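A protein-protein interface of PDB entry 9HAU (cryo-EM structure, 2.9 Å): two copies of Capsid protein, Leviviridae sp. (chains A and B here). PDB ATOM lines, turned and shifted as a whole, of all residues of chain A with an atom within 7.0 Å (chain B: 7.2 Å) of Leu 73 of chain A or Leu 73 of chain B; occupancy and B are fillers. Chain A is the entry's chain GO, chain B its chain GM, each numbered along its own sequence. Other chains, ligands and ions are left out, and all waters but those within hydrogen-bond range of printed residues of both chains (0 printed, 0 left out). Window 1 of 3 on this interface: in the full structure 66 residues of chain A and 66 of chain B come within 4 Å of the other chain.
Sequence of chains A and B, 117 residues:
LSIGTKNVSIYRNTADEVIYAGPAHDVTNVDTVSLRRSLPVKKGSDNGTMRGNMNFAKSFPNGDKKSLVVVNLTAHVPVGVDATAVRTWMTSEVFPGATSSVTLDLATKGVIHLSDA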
ATOM      1  N   SER A  34     -26.324 -23.514   1.523  1.00  0.00           N
ATOM      2  CA  SER A  34     -25.365 -24.319   2.261  1.00  0.00           C
ATOM      3  C   SER A  34     -24.035 -23.589   2.376  1.00  0.00           C
ATOM      4  O   SER A  34     -23.535 -23.025   1.400  1.00  0.00           O
ATOM      5  CB  SER A  34     -25.156 -25.672   1.581  1.00  0.00           C
ATOM      6  OG  SER A  34     -26.100 -26.623   2.034  1.00  0.00           O
ATOM      7  N   ARG A  36     -20.347 -24.638   3.309  1.00  0.00           N
ATOM      8  CA  ARG A  36     -19.434 -25.747   3.523  1.00  0.00           C
ATOM      9  C   ARG A  36     -18.003 -25.236   3.488  1.00  0.00           C
ATOM     10  O   ARG A  36     -17.676 -24.303   2.750  1.00  0.00           O
ATOM     11  CB  ARG A  36     -19.624 -26.839   2.466  1.00  0.00           C
ATOM     12  CG  ARG A  36     -19.060 -28.189   2.867  1.00  0.00           C
ATOM     13  CD  ARG A  36     -19.500 -29.281   1.908  1.00  0.00           C
ATOM     14  NE  ARG A  36     -19.383 -28.872   0.515  1.00  0.00           N
ATOM     15  CZ  ARG A  36     -18.307 -29.066  -0.236  1.00  0.00           C
ATOM     16  NH1 ARG A  36     -17.228 -29.660   0.246  1.00  0.00           N
ATOM     17  NH2 ARG A  36     -18.316 -28.658  -1.501  1.00  0.00           N
ATOM     18  N   GLY A  52     -13.850 -22.682   0.715  1.00  0.00           N
ATOM     19  CA  GLY A  52     -15.149 -22.255   1.190  1.00  0.00           C
ATOM     20  C   GLY A  52     -16.192 -22.313   0.096  1.00  0.00           C
ATOM     21  O   GLY A  52     -16.082 -21.605  -0.908  1.00  0.00           O
ATOM     22  N   ASN A  53     -17.212 -23.147   0.274  1.00  0.00           N
ATOM     23  CA  ASN A  53     -18.234 -23.362  -0.741  1.00  0.00           C
ATOM     24  C   ASN A  53     -19.554 -22.774  -0.268  1.00  0.00           C
ATOM     25  O   ASN A  53     -19.984 -23.028   0.861  1.00  0.00           O
ATOM     26  CB  ASN A  53     -18.403 -24.852  -1.048  1.00  0.00           C
ATOM     27  CG  ASN A  53     -19.534 -25.120  -2.022  1.00  0.00           C
ATOM     28  OD1 ASN A  53     -19.898 -24.262  -2.824  1.00  0.00           O
ATOM     29  ND2 ASN A  53     -20.107 -26.315  -1.945  1.00  0.00           N
ATOM     30  N   MET A  54     -20.184 -21.986  -1.131  1.00  0.00           N
ATOM     31  CA  MET A  54     -21.509 -21.435  -0.889  1.00  0.00           C
ATOM     32  C   MET A  54     -22.461 -22.016  -1.925  1.00  0.00           C
ATOM     33  O   MET A  54     -22.341 -21.719  -3.118  1.00  0.00           O
ATOM     34  CB  MET A  54     -21.487 -19.909  -0.963  1.00  0.00           C
ATOM     35  CG  MET A  54     -22.585 -19.240  -0.176  1.00  0.00           C
ATOM     36  SD  MET A  54     -22.425 -17.451  -0.157  1.00  0.00           S
ATOM     37  CE  MET A  54     -23.893 -17.009   0.755  1.00  0.00           C
ATOM     38  N   ASN A  55     -23.400 -22.838  -1.470  1.00  0.00           N
ATOM     39  CA  ASN A  55     -24.304 -23.566  -2.346  1.00  0.00           C
ATOM     40  C   ASN A  55     -25.705 -22.980  -2.250  1.00  0.00           C
ATOM     41  O   ASN A  55     -26.265 -22.877  -1.157  1.00  0.00           O
ATOM     42  CB  ASN A  55     -24.330 -25.052  -1.986  1.00  0.00           C
ATOM     43  CG  ASN A  55     -24.840 -25.917  -3.116  1.00  0.00           C
ATOM     44  OD1 ASN A  55     -26.047 -26.065  -3.304  1.00  0.00           O
ATOM     45  ND2 ASN A  55     -23.923 -26.501  -3.874  1.00  0.00           N
ATOM     46  N   PHE A  56     -26.263 -22.599  -3.395  1.00  0.00           N
ATOM     47  CA  PHE A  56     -27.643 -22.145  -3.499  1.00  0.00           C
ATOM     48  C   PHE A  56     -28.432 -23.199  -4.260  1.00  0.00           C
ATOM     49  O   PHE A  56     -28.059 -23.564  -5.379  1.00  0.00           O
ATOM     50  CB  PHE A  56     -27.741 -20.797  -4.213  1.00  0.00           C
ATOM     51  CG  PHE A  56     -27.014 -19.681  -3.523  1.00  0.00           C
ATOM     52  CD1 PHE A  56     -25.640 -19.551  -3.639  1.00  0.00           C
ATOM     53  CD2 PHE A  56     -27.708 -18.746  -2.775  1.00  0.00           C
ATOM     54  CE1 PHE A  56     -24.975 -18.519  -3.012  1.00  0.00           C
ATOM     55  CE2 PHE A  56     -27.046 -17.713  -2.147  1.00  0.00           C
ATOM     56  CZ  PHE A  56     -25.680 -17.599  -2.266  1.00  0.00           C
ATOM     57  N   VAL A  71     -26.501 -23.088  -7.741  1.00  0.00           N
ATOM     58  CA  VAL A  71     -25.436 -22.119  -7.967  1.00  0.00           C
ATOM     59  C   VAL A  71     -24.405 -22.302  -6.864  1.00  0.00           C
ATOM     60  O   VAL A  71     -24.748 -22.260  -5.678  1.00  0.00           O
ATOM     61  CB  VAL A  71     -25.958 -20.673  -7.988  1.00  0.00           C
ATOM     62  CG1 VAL A  71     -24.798 -19.696  -8.014  1.00  0.00           C
ATOM     63  CG2 VAL A  71     -26.865 -20.456  -9.184  1.00  0.00           C
ATOM     64  N   ASN A  72     -23.150 -22.506  -7.251  1.00  0.00           N
ATOM     65  CA  ASN A  72     -22.058 -22.712  -6.312  1.00  0.00           C
ATOM     66  C   ASN A  72     -21.079 -21.549  -6.380  1.00  0.00           C
ATOM     67  O   ASN A  72     -20.743 -21.071  -7.467  1.00  0.00           O
ATOM     68  CB  ASN A  72     -21.316 -24.018  -6.602  1.00  0.00           C
ATOM     69  CG  ASN A  72     -21.989 -25.217  -5.979  1.00  0.00           C
ATOM     70  OD1 ASN A  72     -22.049 -25.341  -4.759  1.00  0.00           O
ATOM     71  ND2 ASN A  72     -22.497 -26.110  -6.816  1.00  0.00           N
ATOM     72  N   LEU A  73     -20.629 -21.098  -5.214  1.00  0.00           N
ATOM     73  CA  LEU A  73     -19.566 -20.107  -5.100  1.00  0.00           C
ATOM     74  C   LEU A  73     -18.470 -20.706  -4.227  1.00  0.00           C
ATOM     75  O   LEU A  73     -18.680 -20.937  -3.033  1.00  0.00           O
ATOM     76  CB  LEU A  73     -20.091 -18.798  -4.517  1.00  0.00           C
ATOM     77  CG  LEU A  73     -19.154 -17.591  -4.576  1.00  0.00           C
ATOM     78  CD1 LEU A  73     -18.814 -17.239  -6.008  1.00  0.00           C
ATOM     79  CD2 LEU A  73     -19.792 -16.408  -3.887  1.00  0.00           C
ATOM     80  N   THR A  74     -17.308 -20.958  -4.822  1.00  0.00           N
ATOM     81  CA  THR A  74     -16.198 -21.608  -4.140  1.00  0.00           C
ATOM     82  C   THR A  74     -14.965 -20.718  -4.208  1.00  0.00           C
ATOM     83  O   THR A  74     -14.671 -20.139  -5.257  1.00  0.00           O
ATOM     84  CB  THR A  74     -15.890 -22.973  -4.760  1.00  0.00           C
ATOM     85  OG1 THR A  74     -17.113 -23.673  -5.012  1.00  0.00           O
ATOM     86  CG2 THR A  74     -15.029 -23.802  -3.820  1.00  0.00           C
ATOM     87  N   ALA A  75     -14.252 -20.615  -3.090  1.00  0.00           N
ATOM     88  CA  ALA A  75     -13.002 -19.878  -3.015  1.00  0.00           C
ATOM     89  C   ALA A  75     -11.903 -20.792  -2.495  1.00  0.00           C
ATOM     90  O   ALA A  75     -12.139 -21.614  -1.605  1.00  0.00           O
ATOM     91  CB  ALA A  75     -13.132 -18.649  -2.114  1.00  0.00           C
ATOM     92  N   MET A  90     -11.668  -9.534  -3.610  1.00  0.00           N
ATOM     93  CA  MET A  90     -12.972 -10.146  -3.840  1.00  0.00           C
ATOM     94  C   MET A  90     -14.076  -9.103  -3.937  1.00  0.00           C
ATOM     95  O   MET A  90     -14.981  -9.234  -4.769  1.00  0.00           O
ATOM     96  CB  MET A  90     -13.285 -11.143  -2.726  1.00  0.00           C
ATOM     97  CG  MET A  90     -12.682 -12.516  -2.938  1.00  0.00           C
ATOM     98  SD  MET A  90     -12.821 -13.569  -1.482  1.00  0.00           S
ATOM     99  CE  MET A  90     -14.585 -13.860  -1.443  1.00  0.00           C
ATOM    100  N   VAL A  94     -13.963  -9.353  -7.894  1.00  0.00           N
ATOM    101  CA  VAL A  94     -14.707 -10.588  -8.114  1.00  0.00           C
ATOM    102  C   VAL A  94     -16.207 -10.333  -8.062  1.00  0.00           C
ATOM    103  O   VAL A  94     -16.955 -10.765  -8.945  1.00  0.00           O
ATOM    104  CB  VAL A  94     -14.288 -11.655  -7.085  1.00  0.00           C
ATOM    105  CG1 VAL A  94     -15.091 -12.927  -7.290  1.00  0.00           C
ATOM    106  CG2 VAL A  94     -12.802 -11.930  -7.182  1.00  0.00           C
ATOM    107  N   PHE A  95     -16.664  -9.633  -7.024  1.00  0.00           N
ATOM    108  CA  PHE A  95     -18.098  -9.439  -6.823  1.00  0.00           C
ATOM    109  C   PHE A  95     -18.777  -8.688  -7.961  1.00  0.00           C
ATOM    110  O   PHE A  95     -19.838  -9.145  -8.419  1.00  0.00           O
ATOM    111  CB  PHE A  95     -18.332  -8.750  -5.475  1.00  0.00           C
ATOM    112  CG  PHE A  95     -18.124  -9.650  -4.293  1.00  0.00           C
ATOM    113  CD1 PHE A  95     -17.979 -11.015  -4.464  1.00  0.00           C
ATOM    114  CD2 PHE A  95     -18.070  -9.131  -3.011  1.00  0.00           C
ATOM    115  CE1 PHE A  95     -17.785 -11.845  -3.384  1.00  0.00           C
ATOM    116  CE2 PHE A  95     -17.878  -9.959  -1.925  1.00  0.00           C
ATOM    117  CZ  PHE A  95     -17.736 -11.317  -2.112  1.00  0.00           C
ATOM    118  N   GLY A  97     -18.044  -8.523 -11.133  1.00  0.00           N
ATOM    119  CA  GLY A  97     -18.107  -9.355 -12.321  1.00  0.00           C
ATOM    120  C   GLY A  97     -18.941 -10.603 -12.149  1.00  0.00           C
ATOM    121  O   GLY A  97     -19.547 -11.080 -13.114  1.00  0.00           O
ATOM    122  N   ALA A  98     -18.995 -11.146 -10.933  1.00  0.00           N
ATOM    123  CA  ALA A  98     -19.765 -12.356 -10.688  1.00  0.00           C
ATOM    124  C   ALA A  98     -21.267 -12.105 -10.698  1.00  0.00           C
ATOM    125  O   ALA A  98     -22.035 -13.038 -10.946  1.00  0.00           O
ATOM    126  CB  ALA A  98     -19.352 -12.982  -9.357  1.00  0.00           C
ATOM    127  N   THR A  99     -21.702 -10.873 -10.438  1.00  0.00           N
ATOM    128  CA  THR A  99     -23.117 -10.527 -10.423  1.00  0.00           C
ATOM    129  C   THR A  99     -23.492  -9.613 -11.584  1.00  0.00           C
ATOM    130  O   THR A  99     -24.320  -8.712 -11.433  1.00  0.00           O
ATOM    131  CB  THR A  99     -23.496  -9.880  -9.093  1.00  0.00           C
ATOM    132  OG1 THR A  99     -22.718  -8.693  -8.894  1.00  0.00           O
ATOM    133  CG2 THR A  99     -23.233 -10.840  -7.956  1.00  0.00           C
ATOM    134  N   THR A 103     -22.709 -13.350 -16.030  1.00  0.00           N
ATOM    135  CA  THR A 103     -23.109 -14.559 -15.317  1.00  0.00           C
ATOM    136  C   THR A 103     -24.455 -15.071 -15.813  1.00  0.00           C
ATOM    137  O   THR A 103     -24.632 -16.273 -16.038  1.00  0.00           O
ATOM    138  CB  THR A 103     -23.167 -14.290 -13.813  1.00  0.00           C
ATOM    139  OG1 THR A 103     -21.997 -13.571 -13.406  1.00  0.00           O
ATOM    140  CG2 THR A 103     -23.249 -15.596 -13.048  1.00  0.00           C
ATOM    141  N   LEU A 106     -24.103 -16.420 -19.422  1.00  0.00           N
ATOM    142  CA  LEU A 106     -23.412 -17.705 -19.430  1.00  0.00           C
ATOM    143  C   LEU A 106     -24.313 -18.821 -18.914  1.00  0.00           C
ATOM    144  O   LEU A 106     -24.277 -19.943 -19.430  1.00  0.00           O
ATOM    145  CB  LEU A 106     -22.134 -17.611 -18.599  1.00  0.00           C
ATOM    146  CG  LEU A 106     -21.378 -18.906 -18.298  1.00  0.00           C
ATOM    147  CD1 LEU A 106     -20.908 -19.575 -19.582  1.00  0.00           C
ATOM    148  CD2 LEU A 106     -20.207 -18.627 -17.373  1.00  0.00           C
ATOM    149  N   SER B  34     -11.968 -16.473 -16.319  1.00  0.00           N
ATOM    150  CA  SER B  34     -12.234 -17.522 -17.292  1.00  0.00           C
ATOM    151  C   SER B  34     -13.725 -17.826 -17.351  1.00  0.00           C
ATOM    152  O   SER B  34     -14.390 -17.932 -16.317  1.00  0.00           O
ATOM    153  CB  SER B  34     -11.457 -18.793 -16.948  1.00  0.00           C
ATOM    154  OG  SER B  34     -11.589 -19.760 -17.971  1.00  0.00           O
ATOM    155  N   ARG B  36     -16.312 -20.653 -18.816  1.00  0.00           N
ATOM    156  CA  ARG B  36     -16.384 -22.019 -19.308  1.00  0.00           C
ATOM    157  C   ARG B  36     -17.828 -22.486 -19.319  1.00  0.00           C
ATOM    158  O   ARG B  36     -18.599 -22.171 -18.410  1.00  0.00           O
ATOM    159  CB  ARG B  36     -15.537 -22.967 -18.454  1.00  0.00           C
ATOM    160  CG  ARG B  36     -15.352 -24.345 -19.068  1.00  0.00           C
ATOM    161  CD  ARG B  36     -14.151 -25.060 -18.480  1.00  0.00           C
ATOM    162  NE  ARG B  36     -14.507 -25.847 -17.305  1.00  0.00           N
ATOM    163  CZ  ARG B  36     -14.205 -25.508 -16.059  1.00  0.00           C
ATOM    164  NH1 ARG B  36     -13.535 -24.400 -15.788  1.00  0.00           N
ATOM    165  NH2 ARG B  36     -14.586 -26.299 -15.062  1.00  0.00           N
ATOM    166  N   GLY B  52     -22.507 -23.510 -16.441  1.00  0.00           N
ATOM    167  CA  GLY B  52     -21.693 -22.350 -16.738  1.00  0.00           C
ATOM    168  C   GLY B  52     -20.800 -21.967 -15.577  1.00  0.00           C
ATOM    169  O   GLY B  52     -21.291 -21.658 -14.487  1.00  0.00           O
ATOM    170  N   ASN B  53     -19.489 -21.981 -15.794  1.00  0.00           N
ATOM    171  CA  ASN B  53     -18.512 -21.711 -14.749  1.00  0.00           C
ATOM    172  C   ASN B  53     -17.744 -20.438 -15.072  1.00  0.00           C
ATOM    173  O   ASN B  53     -17.220 -20.289 -16.179  1.00  0.00           O
ATOM    174  CB  ASN B  53     -17.540 -22.881 -14.589  1.00  0.00           C
ATOM    175  CG  ASN B  53     -16.497 -22.627 -13.522  1.00  0.00           C
ATOM    176  OD1 ASN B  53     -15.397 -22.159 -13.812  1.00  0.00           O
ATOM    177  ND2 ASN B  53     -16.840 -22.928 -12.277  1.00  0.00           N
ATOM    178  N   MET B  54     -17.673 -19.531 -14.102  1.00  0.00           N
ATOM    179  CA  MET B  54     -16.865 -18.324 -14.205  1.00  0.00           C
ATOM    180  C   MET B  54     -15.762 -18.384 -13.158  1.00  0.00           C
ATOM    181  O   MET B  54     -16.036 -18.572 -11.970  1.00  0.00           O
ATOM    182  CB  MET B  54     -17.719 -17.067 -14.029  1.00  0.00           C
ATOM    183  CG  MET B  54     -16.913 -15.791 -13.895  1.00  0.00           C
ATOM    184  SD  MET B  54     -17.879 -14.283 -14.109  1.00  0.00           S
ATOM    185  CE  MET B  54     -19.433 -14.951 -14.690  1.00  0.00           C
ATOM    186  N   ASN B  55     -14.519 -18.223 -13.603  1.00  0.00           N
ATOM    187  CA  ASN B  55     -13.338 -18.424 -12.775  1.00  0.00           C
ATOM    188  C   ASN B  55     -12.618 -17.100 -12.571  1.00  0.00           C
ATOM    189  O   ASN B  55     -12.447 -16.331 -13.520  1.00  0.00           O
ATOM    190  CB  ASN B  55     -12.394 -19.439 -13.425  1.00  0.00           C
ATOM    191  CG  ASN B  55     -11.660 -20.286 -12.412  1.00  0.00           C
ATOM    192  OD1 ASN B  55     -12.140 -21.339 -12.002  1.00  0.00           O
ATOM    193  ND2 ASN B  55     -10.481 -19.834 -12.009  1.00  0.00           N
ATOM    194  N   PHE B  56     -12.205 -16.834 -11.335  1.00  0.00           N
ATOM    195  CA  PHE B  56     -11.386 -15.675 -11.003  1.00  0.00           C
ATOM    196  C   PHE B  56     -10.087 -16.157 -10.377  1.00  0.00           C
ATOM    197  O   PHE B  56     -10.111 -16.921  -9.407  1.00  0.00           O
ATOM    198  CB  PHE B  56     -12.108 -14.730 -10.041  1.00  0.00           C
ATOM    199  CG  PHE B  56     -13.300 -14.048 -10.638  1.00  0.00           C
ATOM    200  CD1 PHE B  56     -14.530 -14.682 -10.683  1.00  0.00           C
ATOM    201  CD2 PHE B  56     -13.195 -12.769 -11.153  1.00  0.00           C
ATOM    202  CE1 PHE B  56     -15.627 -14.052 -11.227  1.00  0.00           C
ATOM    203  CE2 PHE B  56     -14.289 -12.137 -11.701  1.00  0.00           C
ATOM    204  CZ  PHE B  56     -15.507 -12.780 -11.739  1.00  0.00           C
ATOM    205  N   VAL B  71     -11.495 -18.043  -7.203  1.00  0.00           N
ATOM    206  CA  VAL B  71     -12.906 -17.952  -6.849  1.00  0.00           C
ATOM    207  C   VAL B  71     -13.723 -18.485  -8.017  1.00  0.00           C
ATOM    208  O   VAL B  71     -13.578 -18.015  -9.151  1.00  0.00           O
ATOM    209  CB  VAL B  71     -13.321 -16.512  -6.501  1.00  0.00           C
ATOM    210  CG1 VAL B  71     -14.820 -16.435  -6.281  1.00  0.00           C
ATOM    211  CG2 VAL B  71     -12.580 -16.033  -5.267  1.00  0.00           C
ATOM    212  N   ASN B  72     -14.580 -19.462  -7.737  1.00  0.00           N
ATOM    213  CA  ASN B  72     -15.394 -20.121  -8.747  1.00  0.00           C
ATOM    214  C   ASN B  72     -16.866 -19.807  -8.523  1.00  0.00           C
ATOM    215  O   ASN B  72     -17.341 -19.799  -7.385  1.00  0.00           O
ATOM    216  CB  ASN B  72     -15.181 -21.635  -8.714  1.00  0.00           C
ATOM    217  CG  ASN B  72     -14.269 -22.117  -9.814  1.00  0.00           C
ATOM    218  OD1 ASN B  72     -14.613 -22.046 -10.992  1.00  0.00           O
ATOM    219  ND2 ASN B  72     -13.095 -22.607  -9.439  1.00  0.00           N
ATOM    220  N   LEU B  73     -17.583 -19.550  -9.614  1.00  0.00           N
ATOM    221  CA  LEU B  73     -19.028 -19.350  -9.581  1.00  0.00           C
ATOM    222  C   LEU B  73     -19.645 -20.180 -10.698  1.00  0.00           C
ATOM    223  O   LEU B  73     -19.474 -19.861 -11.877  1.00  0.00           O
ATOM    224  CB  LEU B  73     -19.392 -17.873  -9.730  1.00  0.00           C
ATOM    225  CG  LEU B  73     -20.891 -17.575  -9.767  1.00  0.00           C
ATOM    226  CD1 LEU B  73     -21.531 -17.879  -8.427  1.00  0.00           C
ATOM    227  CD2 LEU B  73     -21.134 -16.133 -10.160  1.00  0.00           C
ATOM    228  N   THR B  74     -20.368 -21.233 -10.328  1.00  0.00           N
ATOM    229  CA  THR B  74     -20.911 -22.193 -11.280  1.00  0.00           C
ATOM    230  C   THR B  74     -22.423 -22.265 -11.139  1.00  0.00           C
ATOM    231  O   THR B  74     -22.947 -22.300 -10.022  1.00  0.00           O
ATOM    232  CB  THR B  74     -20.304 -23.583 -11.067  1.00  0.00           C
ATOM    233  OG1 THR B  74     -18.896 -23.461 -10.834  1.00  0.00           O
ATOM    234  CG2 THR B  74     -20.538 -24.457 -12.288  1.00  0.00           C
ATOM    235  N   ALA B  75     -23.118 -22.295 -12.272  1.00  0.00           N
ATOM    236  CA  ALA B  75     -24.566 -22.432 -12.315  1.00  0.00           C
ATOM    237  C   ALA B  75     -24.929 -23.756 -12.971  1.00  0.00           C
ATOM    238  O   ALA B  75     -24.379 -24.105 -14.018  1.00  0.00           O
ATOM    239  CB  ALA B  75     -25.204 -21.268 -13.077  1.00  0.00           C
ATOM    240  N   MET B  90     -31.615 -15.660  -9.562  1.00  0.00           N
ATOM    241  CA  MET B  90     -30.195 -15.369  -9.393  1.00  0.00           C
ATOM    242  C   MET B  90     -29.967 -13.914  -9.001  1.00  0.00           C
ATOM    243  O   MET B  90     -29.131 -13.622  -8.139  1.00  0.00           O
ATOM    244  CB  MET B  90     -29.437 -15.701 -10.677  1.00  0.00           C
ATOM    245  CG  MET B  90     -29.415 -17.179 -11.019  1.00  0.00           C
ATOM    246  SD  MET B  90     -28.491 -17.531 -12.525  1.00  0.00           S
ATOM    247  CE  MET B  90     -26.811 -17.481 -11.913  1.00  0.00           C
ATOM    248  N   VAL B  94     -29.623 -14.970  -5.190  1.00  0.00           N
ATOM    249  CA  VAL B  94     -28.259 -15.487  -5.168  1.00  0.00           C
ATOM    250  C   VAL B  94     -27.247 -14.349  -5.160  1.00  0.00           C
ATOM    251  O   VAL B  94     -26.321 -14.332  -4.342  1.00  0.00           O
ATOM    252  CB  VAL B  94     -28.028 -16.433  -6.359  1.00  0.00           C
ATOM    253  CG1 VAL B  94     -26.609 -16.970  -6.337  1.00  0.00           C
ATOM    254  CG2 VAL B  94     -29.033 -17.567  -6.332  1.00  0.00           C
ATOM    255  N   PHE B  95     -27.408 -13.385  -6.066  1.00  0.00           N
ATOM    256  CA  PHE B  95     -26.416 -12.320  -6.206  1.00  0.00           C
ATOM    257  C   PHE B  95     -26.245 -11.485  -4.943  1.00  0.00           C
ATOM    258  O   PHE B  95     -25.092 -11.245  -4.546  1.00  0.00           O
ATOM    259  CB  PHE B  95     -26.766 -11.448  -7.416  1.00  0.00           C
ATOM    260  CG  PHE B  95     -26.416 -12.073  -8.737  1.00  0.00           C
ATOM    261  CD1 PHE B  95     -25.780 -13.301  -8.790  1.00  0.00           C
ATOM    262  CD2 PHE B  95     -26.724 -11.432  -9.924  1.00  0.00           C
ATOM    263  CE1 PHE B  95     -25.459 -13.876 -10.000  1.00  0.00           C
ATOM    264  CE2 PHE B  95     -26.404 -12.005 -11.137  1.00  0.00           C
ATOM    265  CZ  PHE B  95     -25.771 -13.228 -11.175  1.00  0.00           C
ATOM    266  N   GLY B  97     -26.742 -12.420  -1.872  1.00  0.00           N
ATOM    267  CA  GLY B  97     -26.154 -13.266  -0.850  1.00  0.00           C
ATOM    268  C   GLY B  97     -24.739 -13.703  -1.153  1.00  0.00           C
ATOM    269  O   GLY B  97     -23.959 -13.958  -0.232  1.00  0.00           O
ATOM    270  N   ALA B  98     -24.382 -13.788  -2.432  1.00  0.00           N
ATOM    271  CA  ALA B  98     -23.051 -14.211  -2.842  1.00  0.00           C
ATOM    272  C   ALA B  98     -22.040 -13.074  -2.837  1.00  0.00           C
ATOM    273  O   ALA B  98     -20.859 -13.312  -3.106  1.00  0.00           O
ATOM    274  CB  ALA B  98     -23.104 -14.845  -4.235  1.00  0.00           C
ATOM    275  N   THR B  99     -22.472 -11.847  -2.545  1.00  0.00           N
ATOM    276  CA  THR B  99     -21.578 -10.700  -2.465  1.00  0.00           C
ATOM    277  C   THR B  99     -21.627 -10.039  -1.095  1.00  0.00           C
ATOM    278  O   THR B  99     -21.149  -8.912  -0.934  1.00  0.00           O
ATOM    279  CB  THR B  99     -21.913  -9.680  -3.554  1.00  0.00           C
ATOM    280  OG1 THR B  99     -23.316  -9.397  -3.529  1.00  0.00           O
ATOM    281  CG2 THR B  99     -21.543 -10.228  -4.913  1.00  0.00           C
ATOM    282  N   THR B 103     -20.025 -14.300   2.380  1.00  0.00           N
ATOM    283  CA  THR B 103     -19.073 -14.882   1.440  1.00  0.00           C
ATOM    284  C   THR B 103     -17.641 -14.519   1.814  1.00  0.00           C
ATOM    285  O   THR B 103     -16.739 -15.363   1.760  1.00  0.00           O
ATOM    286  CB  THR B 103     -19.393 -14.419   0.018  1.00  0.00           C
ATOM    287  OG1 THR B 103     -20.689 -14.898  -0.358  1.00  0.00           O
ATOM    288  CG2 THR B 103     -18.360 -14.947  -0.959  1.00  0.00           C
ATOM    289  N   LEU B 106     -16.553 -16.582   4.878  1.00  0.00           N
ATOM    290  CA  LEU B 106     -16.361 -17.996   4.573  1.00  0.00           C
ATOM    291  C   LEU B 106     -15.054 -18.228   3.825  1.00  0.00           C
ATOM    292  O   LEU B 106     -14.343 -19.204   4.090  1.00  0.00           O
ATOM    293  CB  LEU B 106     -17.547 -18.520   3.763  1.00  0.00           C
ATOM    294  CG  LEU B 106     -17.470 -19.968   3.272  1.00  0.00           C
ATOM    295  CD1 LEU B 106     -17.277 -20.929   4.432  1.00  0.00           C
ATOM    296  CD2 LEU B 106     -18.708 -20.327   2.476  1.00  0.00           C
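Asn 53 of chain A touches Leu 106 of chain B, and with the chains exchanged Leu 106 of chain A touches Asn 53 of chain B.
Met 54 of chain A touches Thr 103 of chain B, and with the chains exchanged Thr 103 of chain A touches Met 54 of chain B.
Val 71 of chain A touches Thr 74 of chain B, and with the chains exchanged Thr 74 of chain A touches Val 71 of chain B.
Thr 99 of chain A touches its own counterpart, Thr 99 of chain B.
Of the 36 pairs that touch across the chains among the printed residues, 33 have their exchanged pair printed and touching as well.
The backbone NH of Asn 72 of chain B sits at hydrogen-bond distance from the backbone carbonyl oxygen of Thr 74 of chain A.
The backbone carbonyl oxygen (O) of Thr 74 of chain B sits at hydrogen-bond distance from the backbone NH (N) of Asn 72 of chain A, 2.8 Å away.
OG1 of Thr 103 of chain B lies within hydrogen-bond range of SD of Met 54 of chain A, at 3.1 Å.
The backbone carbonyl oxygen (O) of Gly 97 of chain A lies close to the side-chain sulfur (SD) of Met 54 of chain B, at 3.7 Å.
Of the 20 printed residues of chain A, 17 touch a printed residue of chain B.
Printed residues of chain A that touch a printed residue of chain B: Arg 36, Gly 52, Asn 53, Met 54, Phe 56, Val 71, Asn 72, Leu 73, Thr 74, Met 90, Val 94, Phe 95, Gly 97, Ala 98, Thr 99, Thr 103 and Leu 106.
Hydrophobic or aromatic side chains of chain B that line the printed part of chain A: Met 54, Phe 56, Val 71, Leu 73, Val 94, Phe 95, Ala 98 and Leu 106.
Among the printed residues, no Asp or Glu carboxylate lies within 4 Å of a Lys or Arg side-chain nitrogen of the other chain.
Of the printed residues of chain B, Phe 56 of chain A touches Val 94.
Printed residues of chain B within 4 Å of Val 71 of chain A: Leu 73, Thr 74 and Val 94.
Of the printed residues of chain B, Ala 98 of chain A touches Phe 56, Leu 73 and Phe 95.
Of the printed residues of chain B, Thr 99 of chain A touches Phe 95 and Thr 99.
The nearest printed residue of chain A that does not touch Thr 74 of chain B is Leu 73 of chain A (5.1 Å).
N of Asn 53 of chain B lies within hydrogen-bond range of O of Arg 36 of chain B (2.8 Å).
The side-chain amide oxygen of Asn 55 of chain B sits close to the side-chain amide oxygen of Asn 72 of chain B, 2.8 Å away.
N of Ala 75 of chain A sits at hydrogen-bond distance from O of Gly 52 of chain A (3.0 Å).
The backbone NH (N) of Phe 56 of chain A sits at hydrogen-bond distance from the backbone carbonyl oxygen (O) of Val 71 of chain A (2.8 Å).
The side-chain hydroxyl of Thr 99 of chain A lies within hydrogen-bond range of the backbone carbonyl oxygen of Phe 95 of chain A, 3.0 Å away.
The side-chain hydroxyl (OG1) of Thr 103 of chain A lies within hydrogen-bond range of the backbone carbonyl oxygen (O) of Ala 98 of chain A, 2.5 Å away.
Gly 52 of chain A touches Leu 106 of chain B (CA to CG, 3.9 Å).
Val 71 of chain A touches Thr 74 of chain B (CA to O, 3.2 Å).
CD1 of Leu 73 of chain B touches CD1 of Leu 73 of chain A (3.7 Å).
Thr 103 of chain B touches Leu 73 of chain A (CG2 to CD2, 3.6 Å).
Thr 74 of chain A touches Val 71 of chain B (O to CA, 3.2 Å).
Val 71 of chain B touches Val 94 of chain A.
Ala 98 of chain A touches Phe 56 of chain B.
Thr 99 of chain A touches Thr 99 of chain B.
OG1 of Thr 103 of chain A touches CE of Met 54 of chain B (3.2 Å).
Leu 106 of chain A touches Asn 53 of chain B.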
